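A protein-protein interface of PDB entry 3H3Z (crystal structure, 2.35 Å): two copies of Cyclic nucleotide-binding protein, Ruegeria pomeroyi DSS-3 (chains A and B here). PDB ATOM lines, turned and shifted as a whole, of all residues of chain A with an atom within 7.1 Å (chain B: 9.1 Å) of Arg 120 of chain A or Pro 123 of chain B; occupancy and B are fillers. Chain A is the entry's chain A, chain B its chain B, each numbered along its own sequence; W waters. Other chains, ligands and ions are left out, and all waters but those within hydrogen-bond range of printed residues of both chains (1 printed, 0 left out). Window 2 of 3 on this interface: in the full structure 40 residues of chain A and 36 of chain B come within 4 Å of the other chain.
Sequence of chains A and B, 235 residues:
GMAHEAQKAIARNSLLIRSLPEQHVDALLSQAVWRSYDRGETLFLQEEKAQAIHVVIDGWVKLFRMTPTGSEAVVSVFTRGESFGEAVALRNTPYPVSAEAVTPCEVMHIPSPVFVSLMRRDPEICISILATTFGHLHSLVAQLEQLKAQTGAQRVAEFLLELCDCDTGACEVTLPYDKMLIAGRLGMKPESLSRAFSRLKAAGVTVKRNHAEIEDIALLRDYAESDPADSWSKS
The guanidinium group (NE) of Arg 120 of chain A is in salt-bridge range of the side-chain carboxylate (OE2) of Glu 124 of chain B (2.5 Å). The guanidinium group (NE) of Arg 120 of chain B is in salt-bridge range of the side-chain carboxylate (OE2) of Glu 124 of chain A, at 2.9 Å. The side-chain sulfur (SG) of Cys 126 of chain B sits close to the backbone carbonyl oxygen (O) of Cys 126 of chain A. SG of Cys 126 of chain A lies within hydrogen-bond range of N of Ile 127 of chain B.
Water W1 bridges NE of Arg 91 of chain A (2.8 Å) and O of Ser 128 of chain B (2.9 Å).
Phe 115 of chain A touches none of the printed residues of chain B. Printed residues of chain B within 4 Å of Met 119 of chain A: Pro 123 (3.7 Å) and Leu 130 (3.7 Å). Of chain B, only Pro 123, Glu 124 and Ile 127 come within 4 Å of Arg 120 of chain A. Of the printed residues of chain B, Glu 124 of chain A touches Arg 120. Leu 118 of chain B touches none of the printed residues of chain A. Printed residues of chain A within 4 Å of Met 119 of chain B: Pro 123 (3.7 Å). Pro 123 of chain B touches just these residues of chain A: Met 119 and Arg 120. Of the printed residues of chain A, Cys 126 of chain B touches Cys 126. Of the printed residues of chain A, Ile 127 of chain B touches Leu 90, Arg 120 and Cys 126. The nearest residue of chain B that does not touch Arg 120 of chain A is Asp 122 of chain B (7.2 Å). The nearest printed residue of chain B that does not touch Arg 91 of chain A is Ser 128 of chain B (4.9 Å).
Among the printed residues, pairs that only touch across the chains: Arg 120 of chain A with Pro 123 of chain B (3.6 Å), Arg 91 of chain A with Ala 131 of chain B (3.6 Å), Leu 90 of chain A with Ile 127 of chain B (3.6 Å), Cys 126 of chain A with Leu 130 of chain B (3.7 Å), Met 119 of chain A with Pro 123 of chain B (3.7 Å), Pro 123 of chain A with Met 119 of chain B (3.7 Å), Arg 120 of chain A with Ile 127 of chain B (3.7 Å), Met 119 of chain A with Leu 130 of chain B (3.7 Å), Leu 90 of chain A with Ala 131 of chain B (3.8 Å) and Pro 123 of chain A with Arg 120 of chain B (3.99 Å).
Met 119 of chain A touches Pro 123 of chain B, and with the chains exchanged Pro 123 of chain A touches Met 119 of chain B. Arg 120 of chain A touches Pro 123 of chain B, and with the chains exchanged Pro 123 of chain A touches Arg 120 of chain B. Arg 120 of chain A touches Glu 124 of chain B, and with the chains exchanged Glu 124 of chain A touches Arg 120 of chain B. Cys 126 of chain A touches its own counterpart, Cys 126 of chain B.
Of the 17 printed residues of chain B, 8 touch a printed residue of chain A. Printed residues of chain B that touch a printed residue of chain A: Met 119, Arg 120, Pro 123, Glu 124, Cys 126, Ile 127, Leu 130 and Ala 131. Along chain B the printed residues that touch a printed residue of chain A span positions 119 to 131. Hydrophobic or aromatic side chains of chain A that line the printed part of chain B: Leu 90, Met 119 and Pro 123. Among the printed residues, Asp or Glu carboxylates within 4 Å of a Lys or Arg side-chain nitrogen of the other chain: Arg 120 of chain A with Glu 124 of chain B and Glu 124 of chain A with Arg 120 of chain B.
N of Glu 124 of chain A lies within hydrogen-bond range of OD1 of Asp 122 of chain A (3.0 Å). The side-chain carboxylate (OD1) of Asp 122 of chain B lies close to the backbone NH (N) of Glu 124 of chain B, 3.2 Å away.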
ATOM      1  N   LEU A  90      -7.740  21.147  19.815  1.00  0.00           N
ATOM      2  CA  LEU A  90      -6.339  21.526  19.806  1.00  0.00           C
ATOM      3  C   LEU A  90      -5.658  21.256  18.456  1.00  0.00           C
ATOM      4  O   LEU A  90      -4.769  22.000  18.070  1.00  0.00           O
ATOM      5  CB  LEU A  90      -5.598  20.839  20.918  1.00  0.00           C
ATOM      6  CG  LEU A  90      -5.845  21.266  22.366  1.00  0.00           C
ATOM      7  CD1 LEU A  90      -5.158  20.273  23.327  1.00  0.00           C
ATOM      8  CD2 LEU A  90      -5.331  22.669  22.622  1.00  0.00           C
ATOM      9  N   ARG A  91      -6.035  20.199  17.752  1.00  0.00           N
ATOM     10  CA  ARG A  91      -5.504  19.953  16.412  1.00  0.00           C
ATOM     11  C   ARG A  91      -6.192  20.774  15.311  1.00  0.00           C
ATOM     12  O   ARG A  91      -5.669  20.898  14.220  1.00  0.00           O
ATOM     13  CB  ARG A  91      -5.693  18.510  16.063  1.00  0.00           C
ATOM     14  CG  ARG A  91      -4.875  17.612  16.885  1.00  0.00           C
ATOM     15  CD  ARG A  91      -5.322  16.191  16.725  1.00  0.00           C
ATOM     16  NE  ARG A  91      -4.425  15.332  17.494  1.00  0.00           N
ATOM     17  CZ  ARG A  91      -4.732  14.112  17.920  1.00  0.00           C
ATOM     18  NH1 ARG A  91      -5.945  13.603  17.726  1.00  0.00           N
ATOM     19  NH2 ARG A  91      -3.840  13.431  18.625  1.00  0.00           N
ATOM     20  N   ASN A  92      -7.372  21.313  15.605  1.00  0.00           N
ATOM     21  CA  ASN A  92      -8.198  22.031  14.640  1.00  0.00           C
ATOM     22  C   ASN A  92      -8.539  21.181  13.405  1.00  0.00           C
ATOM     23  O   ASN A  92      -8.472  21.623  12.260  1.00  0.00           O
ATOM     24  CB  ASN A  92      -7.589  23.362  14.229  1.00  0.00           C
ATOM     25  CG  ASN A  92      -8.544  24.189  13.383  1.00  0.00           C
ATOM     26  OD1 ASN A  92      -9.772  24.104  13.519  1.00  0.00           O
ATOM     27  ND2 ASN A  92      -7.991  24.955  12.473  1.00  0.00           N
ATOM     28  N   PRO A 113     -10.457  28.946  20.271  1.00  0.00           N
ATOM     29  CA  PRO A 113      -9.462  30.002  20.237  1.00  0.00           C
ATOM     30  C   PRO A 113      -9.084  30.528  21.608  1.00  0.00           C
ATOM     31  O   PRO A 113      -7.933  30.909  21.800  1.00  0.00           O
ATOM     32  CB  PRO A 113     -10.158  31.096  19.414  1.00  0.00           C
ATOM     33  CG  PRO A 113     -11.087  30.331  18.491  1.00  0.00           C
ATOM     34  CD  PRO A 113     -11.651  29.333  19.489  1.00  0.00           C
ATOM     35  N   PHE A 115      -8.939  28.750  24.462  1.00  0.00           N
ATOM     36  CA  PHE A 115      -8.058  27.763  25.067  1.00  0.00           C
ATOM     37  C   PHE A 115      -6.729  27.595  24.308  1.00  0.00           C
ATOM     38  O   PHE A 115      -5.664  27.538  24.927  1.00  0.00           O
ATOM     39  CB  PHE A 115      -8.784  26.420  25.165  1.00  0.00           C
ATOM     40  CG  PHE A 115      -8.032  25.397  25.907  1.00  0.00           C
ATOM     41  CD1 PHE A 115      -7.959  25.450  27.278  1.00  0.00           C
ATOM     42  CD2 PHE A 115      -7.385  24.372  25.256  1.00  0.00           C
ATOM     43  CE1 PHE A 115      -7.250  24.513  27.974  1.00  0.00           C
ATOM     44  CE2 PHE A 115      -6.691  23.403  25.973  1.00  0.00           C
ATOM     45  CZ  PHE A 115      -6.617  23.491  27.328  1.00  0.00           C
ATOM     46  N   VAL A 116      -6.793  27.498  22.986  1.00  0.00           N
ATOM     47  CA  VAL A 116      -5.585  27.345  22.173  1.00  0.00           C
ATOM     48  C   VAL A 116      -4.680  28.579  22.237  1.00  0.00           C
ATOM     49  O   VAL A 116      -3.446  28.466  22.354  1.00  0.00           O
ATOM     50  CB  VAL A 116      -5.910  27.084  20.696  1.00  0.00           C
ATOM     51  CG1 VAL A 116      -4.643  27.334  19.829  1.00  0.00           C
ATOM     52  CG2 VAL A 116      -6.513  25.676  20.504  1.00  0.00           C
ATOM     53  N   SER A 117      -5.293  29.753  22.203  1.00  0.00           N
ATOM     54  CA  SER A 117      -4.514  30.985  22.195  1.00  0.00           C
ATOM     55  C   SER A 117      -3.785  31.137  23.499  1.00  0.00           C
ATOM     56  O   SER A 117      -2.685  31.601  23.497  1.00  0.00           O
ATOM     57  CB  SER A 117      -5.372  32.232  21.903  1.00  0.00           C
ATOM     58  OG  SER A 117      -6.103  32.597  23.042  1.00  0.00           O
ATOM     59  N   LEU A 118      -4.404  30.743  24.601  1.00  0.00           N
ATOM     60  CA  LEU A 118      -3.771  30.790  25.927  1.00  0.00           C
ATOM     61  C   LEU A 118      -2.437  30.064  25.909  1.00  0.00           C
ATOM     62  O   LEU A 118      -1.424  30.532  26.447  1.00  0.00           O
ATOM     63  CB  LEU A 118      -4.680  30.144  26.983  1.00  0.00           C
ATOM     64  CG  LEU A 118      -4.206  30.063  28.439  1.00  0.00           C
ATOM     65  CD1 LEU A 118      -4.093  31.424  29.049  1.00  0.00           C
ATOM     66  CD2 LEU A 118      -5.151  29.200  29.272  1.00  0.00           C
ATOM     67  N   MET A 119      -2.444  28.927  25.243  1.00  0.00           N
ATOM     68  CA  MET A 119      -1.265  28.083  25.143  1.00  0.00           C
ATOM     69  C   MET A 119      -0.264  28.512  24.090  1.00  0.00           C
ATOM     70  O   MET A 119       0.929  28.322  24.303  1.00  0.00           O
ATOM     71  CB  MET A 119      -1.766  26.685  24.937  1.00  0.00           C
ATOM     72  CG  MET A 119      -2.578  26.383  26.236  1.00  0.00           C
ATOM     73  SD  MET A 119      -2.904  24.628  26.524  1.00  0.00           S
ATOM     74  CE  MET A 119      -3.641  24.354  24.711  1.00  0.00           C
ATOM     75  N   ARG A 120      -0.725  29.131  23.000  1.00  0.00           N
ATOM     76  CA  ARG A 120       0.212  29.700  22.055  1.00  0.00           C
ATOM     77  C   ARG A 120       0.949  30.837  22.728  1.00  0.00           C
ATOM     78  O   ARG A 120       2.133  30.973  22.525  1.00  0.00           O
ATOM     79  CB  ARG A 120      -0.476  30.176  20.798  1.00  0.00           C
ATOM     80  CG  ARG A 120      -0.715  29.070  19.879  1.00  0.00           C
ATOM     81  CD  ARG A 120      -1.637  29.405  18.752  1.00  0.00           C
ATOM     82  NE  ARG A 120      -1.744  28.223  17.929  1.00  0.00           N
ATOM     83  CZ  ARG A 120      -2.686  28.006  17.015  1.00  0.00           C
ATOM     84  NH1 ARG A 120      -3.665  28.881  16.794  1.00  0.00           N
ATOM     85  NH2 ARG A 120      -2.667  26.857  16.335  1.00  0.00           N
ATOM     86  N   ARG A 121       0.271  31.605  23.569  1.00  0.00           N
ATOM     87  CA  ARG A 121       0.886  32.747  24.249  1.00  0.00           C
ATOM     88  C   ARG A 121       1.958  32.428  25.273  1.00  0.00           C
ATOM     89  O   ARG A 121       2.963  33.120  25.360  1.00  0.00           O
ATOM     90  CB  ARG A 121      -0.176  33.580  24.994  1.00  0.00           C
ATOM     91  CG  ARG A 121      -1.055  34.418  24.075  1.00  0.00           C
ATOM     92  CD  ARG A 121      -1.808  35.513  24.878  1.00  0.00           C
ATOM     93  NE  ARG A 121      -2.580  34.972  26.004  1.00  0.00           N
ATOM     94  CZ  ARG A 121      -3.839  34.514  25.947  1.00  0.00           C
ATOM     95  NH1 ARG A 121      -4.542  34.501  24.814  1.00  0.00           N
ATOM     96  NH2 ARG A 121      -4.399  34.045  27.064  1.00  0.00           N
ATOM     97  N   ASP A 122       1.698  31.426  26.094  1.00  0.00           N
ATOM     98  CA  ASP A 122       2.584  31.113  27.192  1.00  0.00           C
ATOM     99  C   ASP A 122       2.860  29.616  27.260  1.00  0.00           C
ATOM    100  O   ASP A 122       2.039  28.839  27.761  1.00  0.00           O
ATOM    101  CB  ASP A 122       1.927  31.621  28.454  1.00  0.00           C
ATOM    102  CG  ASP A 122       2.804  31.533  29.643  1.00  0.00           C
ATOM    103  OD1 ASP A 122       3.873  30.879  29.579  1.00  0.00           O
ATOM    104  OD2 ASP A 122       2.399  32.158  30.661  1.00  0.00           O
ATOM    105  N   PRO A 123       4.006  29.205  26.711  1.00  0.00           N
ATOM    106  CA  PRO A 123       4.422  27.803  26.719  1.00  0.00           C
ATOM    107  C   PRO A 123       4.478  27.196  28.095  1.00  0.00           C
ATOM    108  O   PRO A 123       4.311  26.003  28.221  1.00  0.00           O
ATOM    109  CB  PRO A 123       5.851  27.849  26.133  1.00  0.00           C
ATOM    110  CG  PRO A 123       5.855  29.040  25.299  1.00  0.00           C
ATOM    111  CD  PRO A 123       5.002  30.049  26.033  1.00  0.00           C
ATOM    112  N   GLU A 124       4.709  28.000  29.118  1.00  0.00           N
ATOM    113  CA  GLU A 124       4.750  27.475  30.457  1.00  0.00           C
ATOM    114  C   GLU A 124       3.414  26.862  30.855  1.00  0.00           C
ATOM    115  O   GLU A 124       3.366  25.902  31.626  1.00  0.00           O
ATOM    116  CB  GLU A 124       5.093  28.578  31.449  1.00  0.00           C
ATOM    117  CG  GLU A 124       6.473  29.247  31.249  1.00  0.00           C
ATOM    118  CD  GLU A 124       7.587  28.244  31.138  1.00  0.00           C
ATOM    119  OE1 GLU A 124       7.929  27.593  32.149  1.00  0.00           O
ATOM    120  OE2 GLU A 124       8.114  28.096  30.029  1.00  0.00           O
ATOM    121  N   CYS A 126       1.178  25.411  28.713  1.00  0.00           N
ATOM    122  CA  CYS A 126       1.029  24.136  28.036  1.00  0.00           C
ATOM    123  C   CYS A 126       1.930  23.037  28.645  1.00  0.00           C
ATOM    124  O   CYS A 126       1.505  21.894  28.761  1.00  0.00           O
ATOM    125  CB  CYS A 126       1.305  24.313  26.541  1.00  0.00           C
ATOM    126  SG  CYS A 126       0.706  22.969  25.556  1.00  0.00           S
ATOM    127  N   PRO B  21       4.908  14.180  18.399  1.00  0.00           N
ATOM    128  CA  PRO B  21       4.672  14.243  16.978  1.00  0.00           C
ATOM    129  C   PRO B  21       5.767  13.404  16.336  1.00  0.00           C
ATOM    130  O   PRO B  21       6.956  13.670  16.579  1.00  0.00           O
ATOM    131  CB  PRO B  21       4.833  15.735  16.619  1.00  0.00           C
ATOM    132  CG  PRO B  21       5.079  16.491  17.913  1.00  0.00           C
ATOM    133  CD  PRO B  21       5.377  15.475  18.962  1.00  0.00           C
ATOM    134  N   VAL B 116      12.055  20.474  27.199  1.00  0.00           N
ATOM    135  CA  VAL B 116      11.401  21.728  27.569  1.00  0.00           C
ATOM    136  C   VAL B 116      11.701  22.901  26.604  1.00  0.00           C
ATOM    137  O   VAL B 116      10.774  23.635  26.208  1.00  0.00           O
ATOM    138  CB  VAL B 116      11.751  22.120  29.025  1.00  0.00           C
ATOM    139  CG1 VAL B 116      11.229  23.476  29.331  1.00  0.00           C
ATOM    140  CG2 VAL B 116      11.185  21.065  29.995  1.00  0.00           C
ATOM    141  N   SER B 117      12.960  23.049  26.195  1.00  0.00           N
ATOM    142  CA  SER B 117      13.333  24.135  25.291  1.00  0.00           C
ATOM    143  C   SER B 117      12.668  23.983  23.913  1.00  0.00           C
ATOM    144  O   SER B 117      12.364  24.967  23.257  1.00  0.00           O
ATOM    145  CB  SER B 117      14.827  24.183  25.099  1.00  0.00           C
ATOM    146  OG  SER B 117      15.215  22.941  24.584  1.00  0.00           O
ATOM    147  N   LEU B 118      12.452  22.745  23.493  1.00  0.00           N
ATOM    148  CA  LEU B 118      11.732  22.489  22.259  1.00  0.00           C
ATOM    149  C   LEU B 118      10.343  23.126  22.341  1.00  0.00           C
ATOM    150  O   LEU B 118       9.874  23.798  21.411  1.00  0.00           O
ATOM    151  CB  LEU B 118      11.600  20.995  22.074  1.00  0.00           C
ATOM    152  CG  LEU B 118      11.041  20.417  20.794  1.00  0.00           C
ATOM    153  CD1 LEU B 118      11.896  20.810  19.606  1.00  0.00           C
ATOM    154  CD2 LEU B 118      10.949  18.891  20.949  1.00  0.00           C
ATOM    155  N   MET B 119       9.692  22.962  23.487  1.00  0.00           N
ATOM    156  CA  MET B 119       8.328  23.492  23.631  1.00  0.00           C
ATOM    157  C   MET B 119       8.282  24.993  23.882  1.00  0.00           C
ATOM    158  O   MET B 119       7.304  25.646  23.553  1.00  0.00           O
ATOM    159  CB  MET B 119       7.597  22.704  24.706  1.00  0.00           C
ATOM    160  CG  MET B 119       7.299  21.280  24.176  1.00  0.00           C
ATOM    161  SD  MET B 119       6.528  20.183  25.521  1.00  0.00           S
ATOM    162  CE  MET B 119       8.088  20.120  26.671  1.00  0.00           C
ATOM    163  N   ARG B 120       9.345  25.530  24.454  1.00  0.00           N
ATOM    164  CA  ARG B 120       9.454  26.958  24.658  1.00  0.00           C
ATOM    165  C   ARG B 120       9.749  27.697  23.339  1.00  0.00           C
ATOM    166  O   ARG B 120       9.364  28.860  23.167  1.00  0.00           O
ATOM    167  CB  ARG B 120      10.532  27.259  25.670  1.00  0.00           C
ATOM    168  CG  ARG B 120      10.085  26.940  27.050  1.00  0.00           C
ATOM    169  CD  ARG B 120      11.189  27.176  28.016  1.00  0.00           C
ATOM    170  NE  ARG B 120      10.696  27.039  29.370  1.00  0.00           N
ATOM    171  CZ  ARG B 120      11.448  26.822  30.441  1.00  0.00           C
ATOM    172  NH1 ARG B 120      12.766  26.660  30.361  1.00  0.00           N
ATOM    173  NH2 ARG B 120      10.851  26.713  31.607  1.00  0.00           N
ATOM    174  N   ARG B 121      10.433  26.997  22.443  1.00  0.00           N
ATOM    175  CA  ARG B 121      10.757  27.491  21.144  1.00  0.00           C
ATOM    176  C   ARG B 121       9.513  27.456  20.277  1.00  0.00           C
ATOM    177  O   ARG B 121       9.232  28.453  19.576  1.00  0.00           O
ATOM    178  CB  ARG B 121      11.892  26.692  20.473  1.00  0.00           C
ATOM    179  CG  ARG B 121      13.299  27.031  20.975  1.00  0.00           C
ATOM    180  CD  ARG B 121      14.383  26.585  20.006  1.00  0.00           C
ATOM    181  NE  ARG B 121      14.372  25.139  19.790  1.00  0.00           N
ATOM    182  CZ  ARG B 121      14.888  24.220  20.622  1.00  0.00           C
ATOM    183  NH1 ARG B 121      15.487  24.554  21.774  1.00  0.00           N
ATOM    184  NH2 ARG B 121      14.792  22.936  20.303  1.00  0.00           N
ATOM    185  N   ASP B 122       8.756  26.353  20.339  1.00  0.00           N
ATOM    186  CA  ASP B 122       7.550  26.224  19.528  1.00  0.00           C
ATOM    187  C   ASP B 122       6.416  25.640  20.317  1.00  0.00           C
ATOM    188  O   ASP B 122       6.249  24.438  20.370  1.00  0.00           O
ATOM    189  CB  ASP B 122       7.886  25.324  18.351  1.00  0.00           C
ATOM    190  CG  ASP B 122       6.773  25.246  17.324  1.00  0.00           C
ATOM    191  OD1 ASP B 122       5.715  25.915  17.470  1.00  0.00           O
ATOM    192  OD2 ASP B 122       6.990  24.497  16.368  1.00  0.00           O
ATOM    193  N   PRO B 123       5.602  26.480  20.947  1.00  0.00           N
ATOM    194  CA  PRO B 123       4.531  25.870  21.747  1.00  0.00           C
ATOM    195  C   PRO B 123       3.561  24.940  20.963  1.00  0.00           C
ATOM    196  O   PRO B 123       2.840  24.165  21.601  1.00  0.00           O
ATOM    197  CB  PRO B 123       3.784  27.090  22.329  1.00  0.00           C
ATOM    198  CG  PRO B 123       4.107  28.171  21.409  1.00  0.00           C
ATOM    199  CD  PRO B 123       5.528  27.944  21.004  1.00  0.00           C
ATOM    200  N   GLU B 124       3.554  25.028  19.628  1.00  0.00           N
ATOM    201  CA  GLU B 124       2.769  24.136  18.791  1.00  0.00           C
ATOM    202  C   GLU B 124       3.152  22.657  18.980  1.00  0.00           C
ATOM    203  O   GLU B 124       2.328  21.773  18.760  1.00  0.00           O
ATOM    204  CB  GLU B 124       2.922  24.489  17.318  1.00  0.00           C
ATOM    205  CG  GLU B 124       2.383  25.863  16.943  1.00  0.00           C
ATOM    206  CD  GLU B 124       0.877  25.985  17.101  1.00  0.00           C
ATOM    207  OE1 GLU B 124       0.169  24.935  17.022  1.00  0.00           O
ATOM    208  OE2 GLU B 124       0.410  27.142  17.278  1.00  0.00           O
ATOM    209  N   ILE B 125       4.384  22.396  19.387  1.00  0.00           N
ATOM    210  CA  ILE B 125       4.811  21.040  19.665  1.00  0.00           C
ATOM    211  C   ILE B 125       4.019  20.558  20.910  1.00  0.00           C
ATOM    212  O   ILE B 125       3.398  19.490  20.881  1.00  0.00           O
ATOM    213  CB  ILE B 125       6.360  20.945  19.795  1.00  0.00           C
ATOM    214  CG1 ILE B 125       6.996  21.316  18.458  1.00  0.00           C
ATOM    215  CG2 ILE B 125       6.839  19.542  20.187  1.00  0.00           C
ATOM    216  CD1 ILE B 125       8.474  21.420  18.476  1.00  0.00           C
ATOM    217  N   CYS B 126       4.004  21.370  21.958  1.00  0.00           N
ATOM    218  CA  CYS B 126       3.307  21.014  23.186  1.00  0.00           C
ATOM    219  C   CYS B 126       1.802  20.898  22.928  1.00  0.00           C
ATOM    220  O   CYS B 126       1.170  19.937  23.384  1.00  0.00           O
ATOM    221  CB  CYS B 126       3.612  22.036  24.286  1.00  0.00           C
ATOM    222  SG  CYS B 126       2.896  21.659  25.906  1.00  0.00           S
ATOM    223  N   ILE B 127       1.242  21.850  22.177  1.00  0.00           N
ATOM    224  CA  ILE B 127      -0.175  21.797  21.795  1.00  0.00           C
ATOM    225  C   ILE B 127      -0.497  20.446  21.088  1.00  0.00           C
ATOM    226  O   ILE B 127      -1.444  19.790  21.402  1.00  0.00           O
ATOM    227  CB  ILE B 127      -0.585  22.949  20.889  1.00  0.00           C
ATOM    228  CG1 ILE B 127      -0.589  24.264  21.684  1.00  0.00           C
ATOM    229  CG2 ILE B 127      -1.996  22.743  20.315  1.00  0.00           C
ATOM    230  CD1 ILE B 127      -0.867  25.483  20.838  1.00  0.00           C
ATOM    231  N   SER B 128       0.344  20.030  20.164  1.00  0.00           N
ATOM    232  CA  SER B 128       0.216  18.744  19.511  1.00  0.00           C
ATOM    233  C   SER B 128       0.339  17.507  20.454  1.00  0.00           C
ATOM    234  O   SER B 128      -0.348  16.473  20.299  1.00  0.00           O
ATOM    235  CB  SER B 128       1.288  18.669  18.414  1.00  0.00           C
ATOM    236  OG  SER B 128       1.582  17.307  18.114  1.00  0.00           O
ATOM    237  N   ILE B 129       1.244  17.597  21.414  1.00  0.00           N
ATOM    238  CA  ILE B 129       1.479  16.488  22.345  1.00  0.00           C
ATOM    239  C   ILE B 129       0.304  16.369  23.287  1.00  0.00           C
ATOM    240  O   ILE B 129      -0.135  15.285  23.598  1.00  0.00           O
ATOM    241  CB  ILE B 129       2.792  16.665  23.128  1.00  0.00           C
ATOM    242  CG1 ILE B 129       4.009  16.608  22.178  1.00  0.00           C
ATOM    243  CG2 ILE B 129       2.924  15.585  24.162  1.00  0.00           C
ATOM    244  CD1 ILE B 129       5.322  17.235  22.735  1.00  0.00           C
ATOM    245  N   LEU B 130      -0.215  17.512  23.702  1.00  0.00           N
ATOM    246  CA  LEU B 130      -1.327  17.601  24.642  1.00  0.00           C
ATOM    247  C   LEU B 130      -2.637  17.080  24.025  1.00  0.00           C
ATOM    248  O   LEU B 130      -3.487  16.476  24.723  1.00  0.00           O
ATOM    249  CB  LEU B 130      -1.442  19.043  25.114  1.00  0.00           C
ATOM    250  CG  LEU B 130      -2.407  19.449  26.220  1.00  0.00           C
ATOM    251  CD1 LEU B 130      -2.279  18.544  27.504  1.00  0.00           C
ATOM    252  CD2 LEU B 130      -2.212  20.969  26.523  1.00  0.00           C
ATOM    253  N   ALA B 131      -2.800  17.292  22.729  1.00  0.00           N
ATOM    254  CA  ALA B 131      -3.955  16.779  22.012  1.00  0.00           C
ATOM    255  C   ALA B 131      -3.922  15.250  22.120  1.00  0.00           C
ATOM    256  O   ALA B 131      -4.922  14.613  22.390  1.00  0.00           O
ATOM    257  CB  ALA B 131      -3.948  17.242  20.541  1.00  0.00           C
HETATM  258  O   HOH W   1      -1.721  15.778  17.865  1.00  0.00           O
